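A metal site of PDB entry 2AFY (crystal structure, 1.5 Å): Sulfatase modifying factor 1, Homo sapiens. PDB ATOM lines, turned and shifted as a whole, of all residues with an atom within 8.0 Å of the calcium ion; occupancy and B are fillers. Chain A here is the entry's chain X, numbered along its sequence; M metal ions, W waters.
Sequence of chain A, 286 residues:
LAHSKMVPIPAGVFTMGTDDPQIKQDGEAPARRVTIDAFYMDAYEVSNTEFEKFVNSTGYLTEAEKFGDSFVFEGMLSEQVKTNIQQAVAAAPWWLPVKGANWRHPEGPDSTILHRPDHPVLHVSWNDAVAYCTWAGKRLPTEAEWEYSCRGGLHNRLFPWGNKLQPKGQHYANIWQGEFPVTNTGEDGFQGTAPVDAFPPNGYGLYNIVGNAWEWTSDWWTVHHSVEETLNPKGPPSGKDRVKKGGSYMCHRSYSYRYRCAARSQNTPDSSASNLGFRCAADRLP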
ATOM      1  N   HIS A 171     -19.882 -26.431 -15.661  1.00  0.00           N
ATOM      2  CA  HIS A 171     -20.769 -25.335 -15.308  1.00  0.00           C
ATOM      3  C   HIS A 171     -20.938 -25.266 -13.791  1.00  0.00           C
ATOM      4  O   HIS A 171     -21.178 -26.287 -13.146  1.00  0.00           O
ATOM      5  CB  HIS A 171     -22.101 -25.488 -16.011  1.00  0.00           C
ATOM      6  CG  HIS A 171     -22.029 -25.091 -17.452  1.00  0.00           C
ATOM      7  ND1 HIS A 171     -21.913 -23.774 -17.826  1.00  0.00           N
ATOM      8  CD2 HIS A 171     -21.931 -25.821 -18.592  1.00  0.00           C
ATOM      9  CE1 HIS A 171     -21.764 -23.699 -19.138  1.00  0.00           C
ATOM     10  NE2 HIS A 171     -21.778 -24.932 -19.628  1.00  0.00           N
ATOM     11  N   ALA A 173     -22.866 -22.480 -12.361  1.00  0.00           N
ATOM     12  CA  ALA A 173     -24.064 -21.684 -12.110  1.00  0.00           C
ATOM     13  C   ALA A 173     -24.979 -21.703 -13.305  1.00  0.00           C
ATOM     14  O   ALA A 173     -24.554 -21.938 -14.429  1.00  0.00           O
ATOM     15  CB  ALA A 173     -23.700 -20.243 -11.783  1.00  0.00           C
ATOM     16  N   ASN A 174     -26.240 -21.385 -13.051  1.00  0.00           N
ATOM     17  CA  ASN A 174     -27.269 -21.369 -14.082  1.00  0.00           C
ATOM     18  C   ASN A 174     -27.435 -19.933 -14.603  1.00  0.00           C
ATOM     19  O   ASN A 174     -28.102 -19.112 -13.996  1.00  0.00           O
ATOM     20  CB  ASN A 174     -28.578 -21.863 -13.503  1.00  0.00           C
ATOM     21  CG  ASN A 174     -29.694 -21.890 -14.498  1.00  0.00           C
ATOM     22  OD1 ASN A 174     -29.444 -21.850 -15.706  1.00  0.00           O
ATOM     23  ND2 ASN A 174     -30.952 -21.930 -14.012  1.00  0.00           N
ATOM     24  N   ILE A 175     -26.811 -19.671 -15.738  1.00  0.00           N
ATOM     25  CA  ILE A 175     -26.972 -18.434 -16.485  1.00  0.00           C
ATOM     26  C   ILE A 175     -27.390 -18.771 -17.938  1.00  0.00           C
ATOM     27  O   ILE A 175     -27.852 -19.883 -18.212  1.00  0.00           O
ATOM     28  CB  ILE A 175     -25.727 -17.551 -16.375  1.00  0.00           C
ATOM     29  CG1 ILE A 175     -24.506 -18.243 -16.965  1.00  0.00           C
ATOM     30  CG2 ILE A 175     -25.468 -17.209 -14.924  1.00  0.00           C
ATOM     31  CD1 ILE A 175     -23.308 -17.328 -17.065  1.00  0.00           C
ATOM     32  N   TRP A 176     -27.238 -17.836 -18.862  1.00  0.00           N
ATOM     33  CA  TRP A 176     -27.645 -18.059 -20.248  1.00  0.00           C
ATOM     34  C   TRP A 176     -26.460 -18.540 -21.091  1.00  0.00           C
ATOM     35  O   TRP A 176     -25.359 -18.051 -20.909  1.00  0.00           O
ATOM     36  CB  TRP A 176     -28.108 -16.740 -20.826  1.00  0.00           C
ATOM     37  CG  TRP A 176     -28.729 -16.747 -22.207  1.00  0.00           C
ATOM     38  CD1 TRP A 176     -28.089 -16.831 -23.405  1.00  0.00           C
ATOM     39  CD2 TRP A 176     -30.124 -16.632 -22.504  1.00  0.00           C
ATOM     40  NE1 TRP A 176     -28.992 -16.771 -24.438  1.00  0.00           N
ATOM     41  CE2 TRP A 176     -30.261 -16.646 -23.911  1.00  0.00           C
ATOM     42  CE3 TRP A 176     -31.273 -16.497 -21.715  1.00  0.00           C
ATOM     43  CZ2 TRP A 176     -31.497 -16.542 -24.541  1.00  0.00           C
ATOM     44  CZ3 TRP A 176     -32.497 -16.406 -22.340  1.00  0.00           C
ATOM     45  CH2 TRP A 176     -32.600 -16.425 -23.735  1.00  0.00           C
ATOM     46  N   GLN A 177     -26.695 -19.467 -22.017  1.00  0.00           N
ATOM     47  CA  GLN A 177     -25.714 -19.766 -23.052  1.00  0.00           C
ATOM     48  C   GLN A 177     -26.431 -19.610 -24.361  1.00  0.00           C
ATOM     49  O   GLN A 177     -27.603 -19.950 -24.464  1.00  0.00           O
ATOM     50  CB  GLN A 177     -25.155 -21.183 -22.963  1.00  0.00           C
ATOM     51  CG  GLN A 177     -24.334 -21.416 -21.716  1.00  0.00           C
ATOM     52  CD  GLN A 177     -25.185 -21.848 -20.547  1.00  0.00           C
ATOM     53  OE1 GLN A 177     -26.145 -22.643 -20.741  1.00  0.00           O
ATOM     54  NE2 GLN A 177     -24.853 -21.361 -19.338  1.00  0.00           N
ATOM     55  N   ASN A 184     -31.483 -19.607 -26.142  1.00  0.00           N
ATOM     56  CA  ASN A 184     -30.820 -20.154 -24.963  1.00  0.00           C
ATOM     57  C   ASN A 184     -30.598 -21.642 -25.226  1.00  0.00           C
ATOM     58  O   ASN A 184     -31.552 -22.404 -25.378  1.00  0.00           O
ATOM     59  CB  ASN A 184     -31.718 -19.974 -23.724  1.00  0.00           C
ATOM     60  CG  ASN A 184     -31.011 -20.375 -22.417  1.00  0.00           C
ATOM     61  OD1 ASN A 184     -30.000 -21.091 -22.450  1.00  0.00           O
ATOM     62  ND2 ASN A 184     -31.540 -19.920 -21.287  1.00  0.00           N
ATOM     63  N   THR A 185     -29.337 -22.064 -25.326  1.00  0.00           N
ATOM     64  CA  THR A 185     -29.060 -23.414 -25.727  1.00  0.00           C
ATOM     65  C   THR A 185     -29.284 -24.425 -24.621  1.00  0.00           C
ATOM     66  O   THR A 185     -29.333 -25.639 -24.866  1.00  0.00           O
ATOM     67  CB  THR A 185     -27.595 -23.548 -26.165  1.00  0.00           C
ATOM     68  OG1 THR A 185     -26.769 -23.280 -25.031  1.00  0.00           O
ATOM     69  CG2 THR A 185     -27.277 -22.601 -27.301  1.00  0.00           C
ATOM     70  N   GLY A 186     -29.413 -23.956 -23.375  1.00  0.00           N
ATOM     71  CA  GLY A 186     -29.548 -24.865 -22.249  1.00  0.00           C
ATOM     72  C   GLY A 186     -28.335 -25.750 -22.012  1.00  0.00           C
ATOM     73  O   GLY A 186     -28.446 -26.813 -21.401  1.00  0.00           O
ATOM     74  N   GLU A 187     -27.168 -25.275 -22.448  1.00  0.00           N
ATOM     75  CA  GLU A 187     -25.908 -26.010 -22.280  1.00  0.00           C
ATOM     76  C   GLU A 187     -25.655 -26.404 -20.816  1.00  0.00           C
ATOM     77  O   GLU A 187     -25.181 -27.538 -20.537  1.00  0.00           O
ATOM     78  CB  GLU A 187     -24.750 -25.167 -22.816  1.00  0.00           C
ATOM     79  CG  GLU A 187     -23.402 -25.786 -22.692  1.00  0.00           C
ATOM     80  CD  GLU A 187     -22.276 -24.828 -23.023  1.00  0.00           C
ATOM     81  OE1 GLU A 187     -22.478 -23.891 -23.832  1.00  0.00           O
ATOM     82  OE2 GLU A 187     -21.195 -25.048 -22.436  1.00  0.00           O
ATOM     83  N   ASP A 188     -25.942 -25.498 -19.880  1.00  0.00           N
ATOM     84  CA  ASP A 188     -25.713 -25.777 -18.449  1.00  0.00           C
ATOM     85  C   ASP A 188     -26.743 -26.689 -17.788  1.00  0.00           C
ATOM     86  O   ASP A 188     -26.657 -26.994 -16.587  1.00  0.00           O
ATOM     87  CB  ASP A 188     -25.537 -24.480 -17.658  1.00  0.00           C
ATOM     88  CG  ASP A 188     -26.790 -23.621 -17.628  1.00  0.00           C
ATOM     89  OD1 ASP A 188     -27.905 -24.157 -17.870  1.00  0.00           O
ATOM     90  OD2 ASP A 188     -26.647 -22.403 -17.330  1.00  0.00           O
ATOM     91  N   GLY A 189     -27.729 -27.125 -18.582  1.00  0.00           N
ATOM     92  CA  GLY A 189     -28.735 -28.053 -18.093  1.00  0.00           C
ATOM     93  C   GLY A 189     -30.119 -27.485 -17.822  1.00  0.00           C
ATOM     94  O   GLY A 189     -31.066 -28.239 -17.594  1.00  0.00           O
ATOM     95  N   PHE A 190     -30.241 -26.166 -17.889  1.00  0.00           N
ATOM     96  CA  PHE A 190     -31.476 -25.477 -17.494  1.00  0.00           C
ATOM     97  C   PHE A 190     -31.675 -24.233 -18.314  1.00  0.00           C
ATOM     98  O   PHE A 190     -30.807 -23.344 -18.339  1.00  0.00           O
ATOM     99  CB  PHE A 190     -31.398 -25.105 -16.017  1.00  0.00           C
ATOM    100  CG  PHE A 190     -31.179 -26.288 -15.155  1.00  0.00           C
ATOM    101  CD1 PHE A 190     -32.245 -27.066 -14.751  1.00  0.00           C
ATOM    102  CD2 PHE A 190     -29.903 -26.649 -14.772  1.00  0.00           C
ATOM    103  CE1 PHE A 190     -32.028 -28.209 -13.970  1.00  0.00           C
ATOM    104  CE2 PHE A 190     -29.690 -27.780 -13.988  1.00  0.00           C
ATOM    105  CZ  PHE A 190     -30.752 -28.557 -13.614  1.00  0.00           C
ATOM    106  N   GLN A 191     -32.787 -24.163 -19.026  1.00  0.00           N
ATOM    107  CA  GLN A 191     -33.083 -22.949 -19.778  1.00  0.00           C
ATOM    108  C   GLN A 191     -33.694 -21.902 -18.882  1.00  0.00           C
ATOM    109  O   GLN A 191     -33.288 -20.745 -18.890  1.00  0.00           O
ATOM    110  CB  GLN A 191     -33.999 -23.247 -20.940  1.00  0.00           C
ATOM    111  CG  GLN A 191     -33.234 -23.991 -22.020  1.00  0.00           C
ATOM    112  CD  GLN A 191     -34.107 -24.446 -23.133  1.00  0.00           C
ATOM    113  OE1 GLN A 191     -35.101 -25.129 -22.889  1.00  0.00           O
ATOM    114  NE2 GLN A 191     -33.730 -24.114 -24.374  1.00  0.00           N
ATOM    115  N   GLY A 192     -34.691 -22.311 -18.100  1.00  0.00           N
ATOM    116  CA  GLY A 192     -35.237 -21.480 -17.051  1.00  0.00           C
ATOM    117  C   GLY A 192     -34.511 -21.729 -15.725  1.00  0.00           C
ATOM    118  O   GLY A 192     -33.304 -21.917 -15.705  1.00  0.00           O
ATOM    119  N   THR A 193     -35.255 -21.737 -14.626  1.00  0.00           N
ATOM    120  CA  THR A 193     -34.661 -22.036 -13.356  1.00  0.00           C
ATOM    121  C   THR A 193     -34.221 -23.496 -13.220  1.00  0.00           C
ATOM    122  O   THR A 193     -34.660 -24.369 -13.989  1.00  0.00           O
ATOM    123  CB  THR A 193     -35.621 -21.697 -12.176  1.00  0.00           C
ATOM    124  OG1 THR A 193     -36.844 -22.401 -12.350  1.00  0.00           O
ATOM    125  CG2 THR A 193     -35.894 -20.218 -12.154  1.00  0.00           C
ATOM    126  N   ALA A 194     -33.336 -23.726 -12.229  1.00  0.00           N
ATOM    127  CA  ALA A 194     -32.893 -25.040 -11.789  1.00  0.00           C
ATOM    128  C   ALA A 194     -33.356 -25.251 -10.365  1.00  0.00           C
ATOM    129  O   ALA A 194     -33.648 -24.283  -9.651  1.00  0.00           O
ATOM    130  CB  ALA A 194     -31.362 -25.139 -11.821  1.00  0.00           C
ATOM    131  N   PHE A 199     -26.090 -27.429  -8.924  1.00  0.00           N
ATOM    132  CA  PHE A 199     -24.725 -26.875  -9.091  1.00  0.00           C
ATOM    133  C   PHE A 199     -23.905 -26.981  -7.819  1.00  0.00           C
ATOM    134  O   PHE A 199     -24.462 -27.262  -6.761  1.00  0.00           O
ATOM    135  CB  PHE A 199     -24.778 -25.460  -9.662  1.00  0.00           C
ATOM    136  CG  PHE A 199     -25.353 -25.444 -11.068  1.00  0.00           C
ATOM    137  CD1 PHE A 199     -24.570 -25.828 -12.153  1.00  0.00           C
ATOM    138  CD2 PHE A 199     -26.673 -25.114 -11.310  1.00  0.00           C
ATOM    139  CE1 PHE A 199     -25.110 -25.869 -13.440  1.00  0.00           C
ATOM    140  CE2 PHE A 199     -27.194 -25.153 -12.573  1.00  0.00           C
ATOM    141  CZ  PHE A 199     -26.416 -25.538 -13.629  1.00  0.00           C
ATOM    142  N   ASN A 212     -29.374 -18.423 -11.436  1.00  0.00           N
ATOM    143  CA  ASN A 212     -30.656 -19.050 -11.095  1.00  0.00           C
ATOM    144  C   ASN A 212     -31.670 -17.936 -10.887  1.00  0.00           C
ATOM    145  O   ASN A 212     -32.098 -17.360 -11.896  1.00  0.00           O
ATOM    146  CB  ASN A 212     -30.577 -20.078  -9.946  1.00  0.00           C
ATOM    147  CG  ASN A 212     -31.527 -21.260 -10.168  1.00  0.00           C
ATOM    148  OD1 ASN A 212     -31.841 -21.604 -11.318  1.00  0.00           O
ATOM    149  ND2 ASN A 212     -31.976 -21.900  -9.078  1.00  0.00           N
ATOM    150  N   SER A 248     -29.013 -14.130 -12.592  1.00  0.00           N
ATOM    151  CA  SER A 248     -30.047 -15.111 -12.821  1.00  0.00           C
ATOM    152  C   SER A 248     -29.760 -15.956 -14.047  1.00  0.00           C
ATOM    153  O   SER A 248     -28.769 -15.750 -14.762  1.00  0.00           O
ATOM    154  CB  SER A 248     -31.391 -14.419 -13.021  1.00  0.00           C
ATOM    155  OG  SER A 248     -31.492 -13.819 -14.322  1.00  0.00           O
ATOM    156  N   TYR A 249     -30.687 -16.869 -14.319  1.00  0.00           N
ATOM    157  CA  TYR A 249     -30.632 -17.740 -15.498  1.00  0.00           C
ATOM    158  C   TYR A 249     -30.639 -17.006 -16.812  1.00  0.00           C
ATOM    159  O   TYR A 249     -30.384 -17.606 -17.860  1.00  0.00           O
ATOM    160  CB  TYR A 249     -31.777 -18.771 -15.452  1.00  0.00           C
ATOM    161  CG  TYR A 249     -33.175 -18.217 -15.618  1.00  0.00           C
ATOM    162  CD1 TYR A 249     -33.994 -17.968 -14.514  1.00  0.00           C
ATOM    163  CD2 TYR A 249     -33.691 -17.997 -16.877  1.00  0.00           C
ATOM    164  CE1 TYR A 249     -35.295 -17.496 -14.697  1.00  0.00           C
ATOM    165  CE2 TYR A 249     -34.973 -17.495 -17.053  1.00  0.00           C
ATOM    166  CZ  TYR A 249     -35.770 -17.257 -15.965  1.00  0.00           C
ATOM    167  OH  TYR A 249     -37.046 -16.786 -16.168  1.00  0.00           O
ATOM    168  N   MET A 250     -30.994 -15.718 -16.779  1.00  0.00           N
ATOM    169  CA  MET A 250     -31.040 -14.866 -17.986  1.00  0.00           C
ATOM    170  C   MET A 250     -29.714 -14.210 -18.339  1.00  0.00           C
ATOM    171  O   MET A 250     -29.554 -13.690 -19.454  1.00  0.00           O
ATOM    172  CB  MET A 250     -32.121 -13.793 -17.860  1.00  0.00           C
ATOM    173  CG  MET A 250     -33.493 -14.318 -18.026  1.00  0.00           C
ATOM    174  SD  MET A 250     -34.689 -13.060 -17.598  1.00  0.00           S
ATOM    175  CE  MET A 250     -34.433 -11.897 -18.954  1.00  0.00           C
ATOM    176  N   OCS A 251     -28.775 -14.126 -17.403  1.00  0.00           N
ATOM    177  CA  OCS A 251     -27.622 -13.268 -17.653  1.00  0.00           C
ATOM    178  CB  OCS A 251     -26.846 -13.000 -16.389  1.00  0.00           C
ATOM    179  SG  OCS A 251     -27.610 -11.891 -15.236  1.00  0.00           S
ATOM    180  C   OCS A 251     -26.666 -13.894 -18.656  1.00  0.00           C
ATOM    181  O   OCS A 251     -26.471 -15.095 -18.674  1.00  0.00           O
ATOM    182  OD1 OCS A 251     -26.569 -11.559 -14.320  1.00  0.00           O
ATOM    183  OD2 OCS A 251     -28.083 -10.760 -15.978  1.00  0.00           O
ATOM    184  OD3 OCS A 251     -28.771 -12.527 -14.657  1.00  0.00           O
HETATM  185 CA    CA M   1     -29.001 -21.919 -17.983  1.00  0.00          CA
HETATM  186  O   HOH W   1     -28.673 -22.170 -20.314  1.00  0.00           O
HETATM  187  O   HOH W   2     -30.711 -20.244 -18.453  1.00  0.00           O
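The backbone carbonyl oxygen of Asn 174 lies close to the backbone NH of Tyr 249. The backbone carbonyl oxygen of Gly 192 is in hydrogen-bond range of the side-chain amide nitrogen of Asn 174. The side-chain amide oxygen of Asn 212 lies within hydrogen-bond range of the side-chain amide nitrogen of Asn 174 (2.9 Å). ND2 of Asn 174 sits close to N of Ala 194. N of Asp 188 sits at hydrogen-bond distance from OE1 of Gln 177, at 3.0 Å.
The nearest printed residue that does not touch the calcium ion is Gln 177 (4.04 Å).
The side-chain amide oxygen (OD1) of Asn 174 is bound to the calcium ion (2.3 Å). The backbone carbonyl oxygen (O) of Phe 190 is bound to the calcium ion (2.3 Å). The calcium ion is bound by O of Ile 175. Water W1 binds the calcium ion, at 2.4 Å. The calcium ion is bound by water W2, at 2.4 Å. OD2 of Asp 188 is bound to the calcium ion, at 2.5 Å. The calcium ion is bound by OD1 of Asp 188 (2.5 Å). The calcium ion has seven donor atoms within binding distance.
Water W1 lies within hydrogen-bond range of the side-chain amide oxygen (OE1) of Gln 177 (2.6 Å) and the side-chain amide oxygen (OD1) of Asn 184 (2.7 Å). Water W2 lies within hydrogen-bond range of O of Gln 191 (2.7 Å), O of Tyr 249 (2.7 Å) and ND2 of Asn 184 (3.0 Å).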
